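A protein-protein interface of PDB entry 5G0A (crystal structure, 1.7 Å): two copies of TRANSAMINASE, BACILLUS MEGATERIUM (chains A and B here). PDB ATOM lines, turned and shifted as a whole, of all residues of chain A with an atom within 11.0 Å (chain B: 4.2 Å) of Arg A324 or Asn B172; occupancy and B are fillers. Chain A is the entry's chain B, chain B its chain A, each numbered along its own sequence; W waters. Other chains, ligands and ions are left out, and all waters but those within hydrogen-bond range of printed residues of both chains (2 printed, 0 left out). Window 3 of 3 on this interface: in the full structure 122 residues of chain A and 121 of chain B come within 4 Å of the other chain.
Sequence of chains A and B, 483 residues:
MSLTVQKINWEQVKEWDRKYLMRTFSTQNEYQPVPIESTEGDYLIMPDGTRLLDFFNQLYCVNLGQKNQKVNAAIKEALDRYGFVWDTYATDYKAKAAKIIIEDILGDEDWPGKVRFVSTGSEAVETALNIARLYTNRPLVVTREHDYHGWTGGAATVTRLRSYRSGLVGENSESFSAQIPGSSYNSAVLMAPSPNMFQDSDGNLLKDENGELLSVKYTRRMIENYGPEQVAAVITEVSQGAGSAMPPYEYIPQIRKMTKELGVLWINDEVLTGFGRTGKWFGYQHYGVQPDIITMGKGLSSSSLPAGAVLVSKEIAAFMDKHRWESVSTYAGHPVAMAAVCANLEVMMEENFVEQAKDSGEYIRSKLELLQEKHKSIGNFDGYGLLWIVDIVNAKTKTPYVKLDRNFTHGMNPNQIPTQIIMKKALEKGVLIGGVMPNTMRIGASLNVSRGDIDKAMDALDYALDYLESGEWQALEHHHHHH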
ATOM      1  N   LEU A 134      -6.029  -0.915 -24.175  1.00  0.00           N
ATOM      2  CA  LEU A 134      -4.836  -1.725 -23.944  1.00  0.00           C
ATOM      3  C   LEU A 134      -5.188  -3.219 -23.836  1.00  0.00           C
ATOM      4  O   LEU A 134      -4.484  -4.056 -24.422  1.00  0.00           O
ATOM      5  CB  LEU A 134      -4.072  -1.302 -22.694  1.00  0.00           C
ATOM      6  CG  LEU A 134      -3.262   0.007 -22.807  1.00  0.00           C
ATOM      7  CD1 LEU A 134      -2.952   0.552 -21.416  1.00  0.00           C
ATOM      8  CD2 LEU A 134      -1.991  -0.093 -23.669  1.00  0.00           C
ATOM      9  N   ALA A 317      -7.965  -7.177 -14.934  1.00  0.00           N
ATOM     10  CA  ALA A 317      -6.939  -7.046 -13.896  1.00  0.00           C
ATOM     11  C   ALA A 317      -5.781  -8.027 -14.060  1.00  0.00           C
ATOM     12  O   ALA A 317      -4.628  -7.664 -13.897  1.00  0.00           O
ATOM     13  CB  ALA A 317      -7.558  -7.178 -12.512  1.00  0.00           C
ATOM     14  N   ALA A 318      -6.090  -9.280 -14.399  1.00  0.00           N
ATOM     15  CA  ALA A 318      -5.038 -10.286 -14.544  1.00  0.00           C
ATOM     16  C   ALA A 318      -4.093  -9.926 -15.704  1.00  0.00           C
ATOM     17  O   ALA A 318      -2.887 -10.106 -15.605  1.00  0.00           O
ATOM     18  CB  ALA A 318      -5.656 -11.674 -14.749  1.00  0.00           C
ATOM     19  N   PHE A 319      -4.660  -9.361 -16.770  1.00  0.00           N
ATOM     20  CA  PHE A 319      -3.884  -8.915 -17.914  1.00  0.00           C
ATOM     21  C   PHE A 319      -3.000  -7.735 -17.523  1.00  0.00           C
ATOM     22  O   PHE A 319      -1.783  -7.762 -17.725  1.00  0.00           O
ATOM     23  CB  PHE A 319      -4.811  -8.525 -19.064  1.00  0.00           C
ATOM     24  CG  PHE A 319      -4.109  -7.785 -20.177  1.00  0.00           C
ATOM     25  CD1 PHE A 319      -3.420  -8.476 -21.175  1.00  0.00           C
ATOM     26  CD2 PHE A 319      -4.139  -6.386 -20.225  1.00  0.00           C
ATOM     27  CE1 PHE A 319      -2.795  -7.790 -22.210  1.00  0.00           C
ATOM     28  CE2 PHE A 319      -3.500  -5.697 -21.259  1.00  0.00           C
ATOM     29  CZ  PHE A 319      -2.831  -6.401 -22.251  1.00  0.00           C
ATOM     30  N   MET A 320      -3.607  -6.711 -16.926  1.00  0.00           N
ATOM     31  CA  MET A 320      -2.827  -5.524 -16.518  1.00  0.00           C
ATOM     32  C   MET A 320      -1.698  -5.892 -15.562  1.00  0.00           C
ATOM     33  O   MET A 320      -0.575  -5.378 -15.664  1.00  0.00           O
ATOM     34  CB  MET A 320      -3.745  -4.447 -15.919  1.00  0.00           C
ATOM     35  CG  MET A 320      -4.733  -3.884 -16.945  1.00  0.00           C
ATOM     36  SD  MET A 320      -4.006  -2.939 -18.313  1.00  0.00           S
ATOM     37  CE  MET A 320      -3.292  -1.494 -17.508  1.00  0.00           C
ATOM     38  N   ASP A 321      -1.979  -6.838 -14.667  1.00  0.00           N
ATOM     39  CA  ASP A 321      -1.002  -7.303 -13.685  1.00  0.00           C
ATOM     40  C   ASP A 321       0.274  -7.910 -14.269  1.00  0.00           C
ATOM     41  O   ASP A 321       1.299  -7.968 -13.578  1.00  0.00           O
ATOM     42  CB  ASP A 321      -1.642  -8.359 -12.780  1.00  0.00           C
ATOM     43  CG  ASP A 321      -2.427  -7.761 -11.614  1.00  0.00           C
ATOM     44  OD1 ASP A 321      -2.430  -6.523 -11.397  1.00  0.00           O
ATOM     45  OD2 ASP A 321      -3.039  -8.566 -10.887  1.00  0.00           O
ATOM     46  N   LYS A 322       0.211  -8.375 -15.516  1.00  0.00           N
ATOM     47  CA  LYS A 322       1.368  -9.003 -16.162  1.00  0.00           C
ATOM     48  C   LYS A 322       2.348  -7.999 -16.766  1.00  0.00           C
ATOM     49  O   LYS A 322       3.395  -8.392 -17.270  1.00  0.00           O
ATOM     50  CB  LYS A 322       0.921  -9.988 -17.256  1.00  0.00           C
ATOM     51  CG  LYS A 322       0.265 -11.247 -16.716  1.00  0.00           C
ATOM     52  CD  LYS A 322      -0.358 -12.033 -17.862  1.00  0.00           C
ATOM     53  CE  LYS A 322      -1.122 -13.239 -17.322  1.00  0.00           C
ATOM     54  NZ  LYS A 322      -0.233 -14.399 -17.021  1.00  0.00           N
ATOM     55  N   HIS A 323       2.015  -6.710 -16.710  1.00  0.00           N
ATOM     56  CA  HIS A 323       2.836  -5.678 -17.346  1.00  0.00           C
ATOM     57  C   HIS A 323       3.169  -4.547 -16.397  1.00  0.00           C
ATOM     58  O   HIS A 323       2.566  -4.431 -15.312  1.00  0.00           O
ATOM     59  CB  HIS A 323       2.063  -5.118 -18.553  1.00  0.00           C
ATOM     60  CG  HIS A 323       1.625  -6.175 -19.510  1.00  0.00           C
ATOM     61  ND1 HIS A 323       0.346  -6.693 -19.513  1.00  0.00           N
ATOM     62  CD2 HIS A 323       2.312  -6.858 -20.452  1.00  0.00           C
ATOM     63  CE1 HIS A 323       0.256  -7.623 -20.446  1.00  0.00           C
ATOM     64  NE2 HIS A 323       1.430  -7.740 -21.034  1.00  0.00           N
ATOM     65  N   ARG A 324       4.147  -3.735 -16.799  1.00  0.00           N
ATOM     66  CA  ARG A 324       4.470  -2.491 -16.108  1.00  0.00           C
ATOM     67  C   ARG A 324       3.686  -1.388 -16.815  1.00  0.00           C
ATOM     68  O   ARG A 324       3.910  -1.119 -17.992  1.00  0.00           O
ATOM     69  CB  ARG A 324       5.960  -2.186 -16.182  1.00  0.00           C
ATOM     70  CG  ARG A 324       6.804  -3.193 -15.419  1.00  0.00           C
ATOM     71  CD  ARG A 324       8.267  -2.866 -15.543  1.00  0.00           C
ATOM     72  NE  ARG A 324       9.052  -3.752 -14.674  1.00  0.00           N
ATOM     73  CZ  ARG A 324      10.348  -4.002 -14.816  1.00  0.00           C
ATOM     74  NH1 ARG A 324      11.048  -3.477 -15.815  1.00  0.00           N
ATOM     75  NH2 ARG A 324      10.939  -4.801 -13.932  1.00  0.00           N
ATOM     76  N   TRP A 325       2.774  -0.758 -16.083  1.00  0.00           N
ATOM     77  CA  TRP A 325       1.881   0.247 -16.674  1.00  0.00           C
ATOM     78  C   TRP A 325       2.433   1.631 -16.344  1.00  0.00           C
ATOM     79  O   TRP A 325       2.529   1.987 -15.182  1.00  0.00           O
ATOM     80  CB  TRP A 325       0.479   0.091 -16.090  1.00  0.00           C
ATOM     81  CG  TRP A 325      -0.563   0.972 -16.716  1.00  0.00           C
ATOM     82  CD1 TRP A 325      -0.515   1.566 -17.964  1.00  0.00           C
ATOM     83  CD2 TRP A 325      -1.853   1.266 -16.180  1.00  0.00           C
ATOM     84  NE1 TRP A 325      -1.706   2.235 -18.212  1.00  0.00           N
ATOM     85  CE2 TRP A 325      -2.533   2.077 -17.129  1.00  0.00           C
ATOM     86  CE3 TRP A 325      -2.505   0.937 -14.976  1.00  0.00           C
ATOM     87  CZ2 TRP A 325      -3.833   2.561 -16.911  1.00  0.00           C
ATOM     88  CZ3 TRP A 325      -3.802   1.415 -14.751  1.00  0.00           C
ATOM     89  CH2 TRP A 325      -4.459   2.210 -15.728  1.00  0.00           C
ATOM     90  N   GLU A 326       2.804   2.390 -17.378  1.00  0.00           N
ATOM     91  CA  GLU A 326       3.570   3.631 -17.204  1.00  0.00           C
ATOM     92  C   GLU A 326       2.637   4.832 -17.082  1.00  0.00           C
ATOM     93  O   GLU A 326       2.695   5.778 -17.896  1.00  0.00           O
ATOM     94  CB  GLU A 326       4.498   3.823 -18.395  1.00  0.00           C
ATOM     95  CG  GLU A 326       5.591   2.745 -18.460  1.00  0.00           C
ATOM     96  CD  GLU A 326       6.510   2.933 -19.654  1.00  0.00           C
ATOM     97  OE1 GLU A 326       5.991   3.067 -20.770  1.00  0.00           O
ATOM     98  OE2 GLU A 326       7.750   2.919 -19.492  1.00  0.00           O
ATOM     99  N   SER A 327       1.797   4.798 -16.050  1.00  0.00           N
ATOM    100  CA  SER A 327       0.783   5.843 -15.886  1.00  0.00           C
ATOM    101  C   SER A 327       0.865   6.426 -14.490  1.00  0.00           C
ATOM    102  O   SER A 327       0.824   5.685 -13.491  1.00  0.00           O
ATOM    103  CB  SER A 327      -0.608   5.259 -16.137  1.00  0.00           C
ATOM    104  OG  SER A 327      -1.568   6.282 -16.422  1.00  0.00           O
ATOM    105  N   VAL A 328       1.002   7.753 -14.412  1.00  0.00           N
ATOM    106  CA  VAL A 328       1.015   8.400 -13.100  1.00  0.00           C
ATOM    107  C   VAL A 328       0.076   9.600 -13.106  1.00  0.00           C
ATOM    108  O   VAL A 328      -0.039  10.331 -14.108  1.00  0.00           O
ATOM    109  CB  VAL A 328       2.456   8.803 -12.668  1.00  0.00           C
ATOM    110  CG1 VAL A 328       3.102   9.721 -13.703  1.00  0.00           C
ATOM    111  CG2 VAL A 328       2.465   9.428 -11.262  1.00  0.00           C
ATOM    112  N   PHE B  25       3.804   0.846 -12.858  1.00  0.00           N
ATOM    113  CA  PHE B  25       5.274   0.748 -12.930  1.00  0.00           C
ATOM    114  C   PHE B  25       5.850  -0.611 -12.519  1.00  0.00           C
ATOM    115  O   PHE B  25       6.938  -0.972 -12.965  1.00  0.00           O
ATOM    116  CB  PHE B  25       5.960   1.918 -12.215  1.00  0.00           C
ATOM    117  CG  PHE B  25       5.552   3.261 -12.788  1.00  0.00           C
ATOM    118  CD1 PHE B  25       6.140   3.730 -13.957  1.00  0.00           C
ATOM    119  CD2 PHE B  25       4.533   3.998 -12.192  1.00  0.00           C
ATOM    120  CE1 PHE B  25       5.741   4.947 -14.515  1.00  0.00           C
ATOM    121  CE2 PHE B  25       4.112   5.213 -12.739  1.00  0.00           C
ATOM    122  CZ  PHE B  25       4.715   5.681 -13.900  1.00  0.00           C
ATOM    123  N   THR B  27       5.014  -4.900 -12.283  1.00  0.00           N
ATOM    124  CA  THR B  27       4.140  -6.063 -12.428  1.00  0.00           C
ATOM    125  C   THR B  27       3.629  -6.561 -11.067  1.00  0.00           C
ATOM    126  O   THR B  27       4.249  -6.320 -10.059  1.00  0.00           O
ATOM    127  CB  THR B  27       4.826  -7.244 -13.143  1.00  0.00           C
ATOM    128  OG1 THR B  27       5.860  -7.796 -12.298  1.00  0.00           O
ATOM    129  CG2 THR B  27       5.420  -6.812 -14.470  1.00  0.00           C
ATOM    130  N   GLU B  30       6.370  -8.822  -9.365  1.00  0.00           N
ATOM    131  CA  GLU B  30       7.557  -8.173  -8.768  1.00  0.00           C
ATOM    132  C   GLU B  30       7.213  -7.174  -7.649  1.00  0.00           C
ATOM    133  O   GLU B  30       8.098  -6.729  -6.904  1.00  0.00           O
ATOM    134  CB  GLU B  30       8.369  -7.449  -9.836  1.00  0.00           C
ATOM    135  CG  GLU B  30       7.772  -6.122 -10.321  1.00  0.00           C
ATOM    136  CD  GLU B  30       8.521  -5.594 -11.526  1.00  0.00           C
ATOM    137  OE1 GLU B  30       9.741  -5.814 -11.611  1.00  0.00           O
ATOM    138  OE2 GLU B  30       7.910  -4.954 -12.395  1.00  0.00           O
ATOM    139  N   GLY B 167       1.258   3.730 -21.390  1.00  0.00           N
ATOM    140  CA  GLY B 167       1.388   2.442 -22.109  1.00  0.00           C
ATOM    141  C   GLY B 167       1.844   1.300 -21.211  1.00  0.00           C
ATOM    142  O   GLY B 167       2.106   1.471 -20.013  1.00  0.00           O
ATOM    143  N   LEU B 168       1.977   0.123 -21.818  1.00  0.00           N
ATOM    144  CA  LEU B 168       2.460  -1.061 -21.122  1.00  0.00           C
ATOM    145  C   LEU B 168       3.851  -1.427 -21.628  1.00  0.00           C
ATOM    146  O   LEU B 168       4.136  -1.333 -22.834  1.00  0.00           O
ATOM    147  CB  LEU B 168       1.499  -2.220 -21.414  1.00  0.00           C
ATOM    148  CG  LEU B 168       0.063  -2.061 -20.908  1.00  0.00           C
ATOM    149  CD1 LEU B 168      -0.756  -3.291 -21.307  1.00  0.00           C
ATOM    150  CD2 LEU B 168      -0.013  -1.827 -19.391  1.00  0.00           C
ATOM    151  N   VAL B 169       4.709  -1.836 -20.704  1.00  0.00           N
ATOM    152  CA  VAL B 169       6.020  -2.373 -21.073  1.00  0.00           C
ATOM    153  C   VAL B 169       6.238  -3.677 -20.299  1.00  0.00           C
ATOM    154  O   VAL B 169       5.469  -4.006 -19.391  1.00  0.00           O
ATOM    155  CB  VAL B 169       7.178  -1.357 -20.861  1.00  0.00           C
ATOM    156  CG1 VAL B 169       7.001  -0.163 -21.803  1.00  0.00           C
ATOM    157  CG2 VAL B 169       7.264  -0.904 -19.399  1.00  0.00           C
ATOM    158  N   GLY B 170       7.260  -4.436 -20.688  1.00  0.00           N
ATOM    159  CA  GLY B 170       7.510  -5.723 -20.030  1.00  0.00           C
ATOM    160  C   GLY B 170       8.329  -5.679 -18.757  1.00  0.00           C
ATOM    161  O   GLY B 170       8.895  -4.627 -18.353  1.00  0.00           O
ATOM    162  N   GLU B 171       8.395  -6.842 -18.111  1.00  0.00           N
ATOM    163  CA  GLU B 171       9.191  -7.023 -16.908  1.00  0.00           C
ATOM    164  C   GLU B 171      10.614  -7.417 -17.303  1.00  0.00           C
ATOM    165  O   GLU B 171      10.872  -8.583 -17.628  1.00  0.00           O
ATOM    166  CB  GLU B 171       8.571  -8.106 -15.973  1.00  0.00           C
ATOM    167  CG  GLU B 171       9.296  -8.177 -14.619  1.00  0.00           C
ATOM    168  CD  GLU B 171       8.744  -9.192 -13.625  1.00  0.00           C
ATOM    169  OE1 GLU B 171       7.517  -9.362 -13.517  1.00  0.00           O
ATOM    170  OE2 GLU B 171       9.562  -9.791 -12.884  1.00  0.00           O
ATOM    171  N   ASN B 172      11.522  -6.445 -17.274  1.00  0.00           N
ATOM    172  CA  ASN B 172      12.946  -6.640 -17.596  1.00  0.00           C
ATOM    173  C   ASN B 172      13.140  -7.207 -18.992  1.00  0.00           C
ATOM    174  O   ASN B 172      13.993  -8.069 -19.229  1.00  0.00           O
ATOM    175  CB  ASN B 172      13.638  -7.506 -16.532  1.00  0.00           C
ATOM    176  CG  ASN B 172      13.410  -6.987 -15.133  1.00  0.00           C
ATOM    177  OD1 ASN B 172      13.397  -5.776 -14.903  1.00  0.00           O
ATOM    178  ND2 ASN B 172      13.211  -7.896 -14.186  1.00  0.00           N
ATOM    179  N   SER B 173      12.330  -6.715 -19.920  1.00  0.00           N
ATOM    180  CA  SER B 173      12.347  -7.201 -21.287  1.00  0.00           C
ATOM    181  C   SER B 173      11.743  -6.212 -22.278  1.00  0.00           C
ATOM    182  O   SER B 173      11.105  -5.218 -21.890  1.00  0.00           O
ATOM    183  CB  SER B 173      11.569  -8.514 -21.379  1.00  0.00           C
ATOM    184  OG  SER B 173      11.353  -8.846 -22.736  1.00  0.00           O
ATOM    185  N   HIS B 410      10.359   1.838 -19.271  1.00  0.00           N
ATOM    186  CA  HIS B 410      10.463   1.103 -18.014  1.00  0.00           C
ATOM    187  C   HIS B 410      10.524  -0.412 -18.209  1.00  0.00           C
ATOM    188  O   HIS B 410      10.441  -1.169 -17.234  1.00  0.00           O
ATOM    189  CB  HIS B 410       9.334   1.471 -17.062  1.00  0.00           C
ATOM    190  CG  HIS B 410       9.440   2.867 -16.519  1.00  0.00           C
ATOM    191  ND1 HIS B 410       8.780   3.938 -17.086  1.00  0.00           N
ATOM    192  CD2 HIS B 410      10.123   3.362 -15.460  1.00  0.00           C
ATOM    193  CE1 HIS B 410       9.062   5.039 -16.404  1.00  0.00           C
ATOM    194  NE2 HIS B 410       9.872   4.713 -15.407  1.00  0.00           N
ATOM    195  N   GLY B 411      10.654  -0.853 -19.456  1.00  0.00           N
ATOM    196  CA  GLY B 411      10.882  -2.277 -19.750  1.00  0.00           C
ATOM    197  C   GLY B 411      12.272  -2.717 -19.303  1.00  0.00           C
ATOM    198  O   GLY B 411      12.492  -3.910 -19.079  1.00  0.00           O
ATOM    199  N   MET B 412      13.194  -1.754 -19.148  1.00  0.00           N
ATOM    200  CA  MET B 412      14.580  -2.029 -18.689  1.00  0.00           C
ATOM    201  C   MET B 412      14.611  -2.685 -17.320  1.00  0.00           C
ATOM    202  O   MET B 412      13.762  -2.432 -16.480  1.00  0.00           O
ATOM    203  CB  MET B 412      15.379  -0.729 -18.528  1.00  0.00           C
ATOM    204  CG  MET B 412      15.720   0.013 -19.787  1.00  0.00           C
ATOM    205  SD  MET B 412      17.053   1.160 -19.370  1.00  0.00           S
ATOM    206  CE  MET B 412      18.427   0.074 -18.982  1.00  0.00           C
ATOM    207  N   ASN B 413      15.630  -3.494 -17.074  1.00  0.00           N
ATOM    208  CA  ASN B 413      15.917  -3.915 -15.713  1.00  0.00           C
ATOM    209  C   ASN B 413      16.449  -2.767 -14.864  1.00  0.00           C
ATOM    210  O   ASN B 413      17.413  -2.123 -15.261  1.00  0.00           O
ATOM    211  CB  ASN B 413      16.956  -5.044 -15.736  1.00  0.00           C
ATOM    212  CG  ASN B 413      16.967  -5.835 -14.460  1.00  0.00           C
ATOM    213  OD1 ASN B 413      16.918  -5.267 -13.373  1.00  0.00           O
ATOM    214  ND2 ASN B 413      17.030  -7.174 -14.580  1.00  0.00           N
ATOM    215  N   PRO B 414      15.835  -2.518 -13.681  1.00  0.00           N
ATOM    216  CA  PRO B 414      16.326  -1.442 -12.811  1.00  0.00           C
ATOM    217  C   PRO B 414      17.762  -1.672 -12.285  1.00  0.00           C
ATOM    218  O   PRO B 414      18.412  -0.714 -11.875  1.00  0.00           O
ATOM    219  CB  PRO B 414      15.332  -1.418 -11.647  1.00  0.00           C
ATOM    220  CG  PRO B 414      14.556  -2.694 -11.724  1.00  0.00           C
ATOM    221  CD  PRO B 414      14.578  -3.109 -13.176  1.00  0.00           C
HETATM  222  O   HOH W   1       3.990   4.855 -21.706  1.00  0.00           O
HETATM  223  O   HOH W   2       1.928  -1.989 -13.658  1.00  0.00           O
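The side-chain amide oxygen (OD1) of Asn B172 sits at hydrogen-bond distance from the guanidinium group (NH2) of Arg A324 (2.8 Å). The backbone carbonyl oxygen of His B410 is in hydrogen-bond range of the guanidinium group of Arg A324 (2.8 Å). N of Val B169 lies within hydrogen-bond range of O of Arg A324 (2.9 Å). The backbone carbonyl oxygen of Gly B167 sits at hydrogen-bond distance from the backbone NH of Glu A326 (2.9 Å). N of Phe B25 sits at hydrogen-bond distance from O of Trp A325, 2.9 Å away. The guanidinium group of Arg A324 is in salt-bridge range of the side-chain carboxylate of Glu B30 (2.8 Å). ND1 of His B410 sits at hydrogen-bond distance from OE2 of Glu A326, 2.8 Å away. NH1 of Arg A324 is in hydrogen-bond range of O of Met B412.
The backbone NH (N) of Thr B27 is in hydrogen-bond range of the side-chain carboxylate (OE2) of Glu B30 (2.9 Å). The backbone NH (N) of Ser B173 lies within hydrogen-bond range of the backbone carbonyl oxygen (O) of Gly B411 (2.9 Å). OG1 of Thr B27 sits at hydrogen-bond distance from OE1 of Glu B171, 2.6 Å away. O of Gly B411 sits close to N of Asn B172, at 3.3 Å. The backbone carbonyl oxygen (O) of Phe A319 lies within hydrogen-bond range of a ring nitrogen (ND1) of His A323, 3.0 Å away.
Among the printed residues, merely in contact across the chains: Leu A134 with Leu B168 (3.96 Å), Phe A319 with Leu B168 (3.6 Å), Met A320 with Leu B168 (3.8 Å), Asp A321 with Thr B27 (3.6 Å), Lys A322 with Thr B27 (3.8 Å), His A323 with Thr B27 (3.7 Å), His A323 with Leu B168 (3.98 Å), His A323 with Val B169 (3.7 Å), Arg A324 with Phe B25 (3.3 Å), Arg A324 with Thr B27 (3.99 Å), Arg A324 with Gly B167 (3.7 Å), Arg A324 with Leu B168 (3.5 Å), Arg A324 with Gly B170 (3.4 Å), Arg A324 with Glu B171 (3.8 Å), Arg A324 with Gly B411 (3.6 Å), Trp A325 with Gly B167 (3.3 Å), Trp A325 with Leu B168 (3.7 Å), Glu A326 with Phe B25 (3.7 Å), Glu A326 with Val B169 (3.5 Å), Ser A327 with Phe B25 (3.4 Å) and Val A328 with Phe B25 (3.95 Å).
Of the printed residues of chain B, Arg A324 touches Phe B25, Thr B27, Glu B30, Gly B167, Leu B168, Val B169, Gly B170, Glu B171, Asn B172, His B410, Gly B411 and Met B412. Gly B167 touches just these residues of chain A: Arg A324, Trp A325 and Glu A326. Val B169 touches just these residues of chain A: His A323 (3.7 Å), Arg A324 (2.9 Å) and Glu A326 (3.5 Å). Of chain A, only Arg A324 (3.4 Å) comes within 4 Å of Gly B170. Gly B411 touches just one residue of chain A: Arg A324. Printed residues of chain B within 4 Å of Met A320: Leu B168 (3.8 Å). Of the printed residues of chain A, Thr B27 touches Asp A321 (3.6 Å), Lys A322 (3.8 Å), His A323 (3.7 Å) and Arg A324 (3.99 Å). Of the printed residues of chain A, Met B412 touches Arg A324. Printed residues of chain B within 4 Å of Glu A326: Phe B25, Gly B167, Val B169 and His B410. Ala A317 touches none of the printed residues of chain B. The nearest printed residue of chain B that does not touch Arg A324 is Pro B414 (4.1 Å). The nearest printed residue of chain B that does not touch Lys A322 is Val B169 (5.3 Å).
Printed residues of chain B that touch a printed residue of chain A: Phe B25, Thr B27, Glu B30, Gly B167, Leu B168, Val B169, Gly B170, Glu B171, Asn B172, His B410, Gly B411 and Met B412. Hydrophobic or aromatic side chains of chain B that line the printed part of chain A: Phe B25, Leu B168, Val B169 and His B410. Hydrophobic or aromatic side chains of chain A that line the printed part of chain B: Leu A134, Phe A319, Met A320, His A323, Trp A325 and Val A328. Along chain A the printed residues that touch a printed residue of chain B span positions 134 to 328.
No position is printed for both chains. Of the 29 pairs that touch across the chains among the printed residues, none has its exchanged pair printed and touching as well.
Water W1 lies within hydrogen-bond range of the side-chain carboxylate (OE1) of Glu A326 (2.8 Å) and the backbone NH (N) of Gly B167 (3.0 Å). Water W2 lies within hydrogen-bond range of the backbone NH (N) of Trp A325 (2.8 Å), the backbone carbonyl oxygen (O) of His A323 (3.0 Å) and the backbone NH (N) of Phe B25 (3.5 Å).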
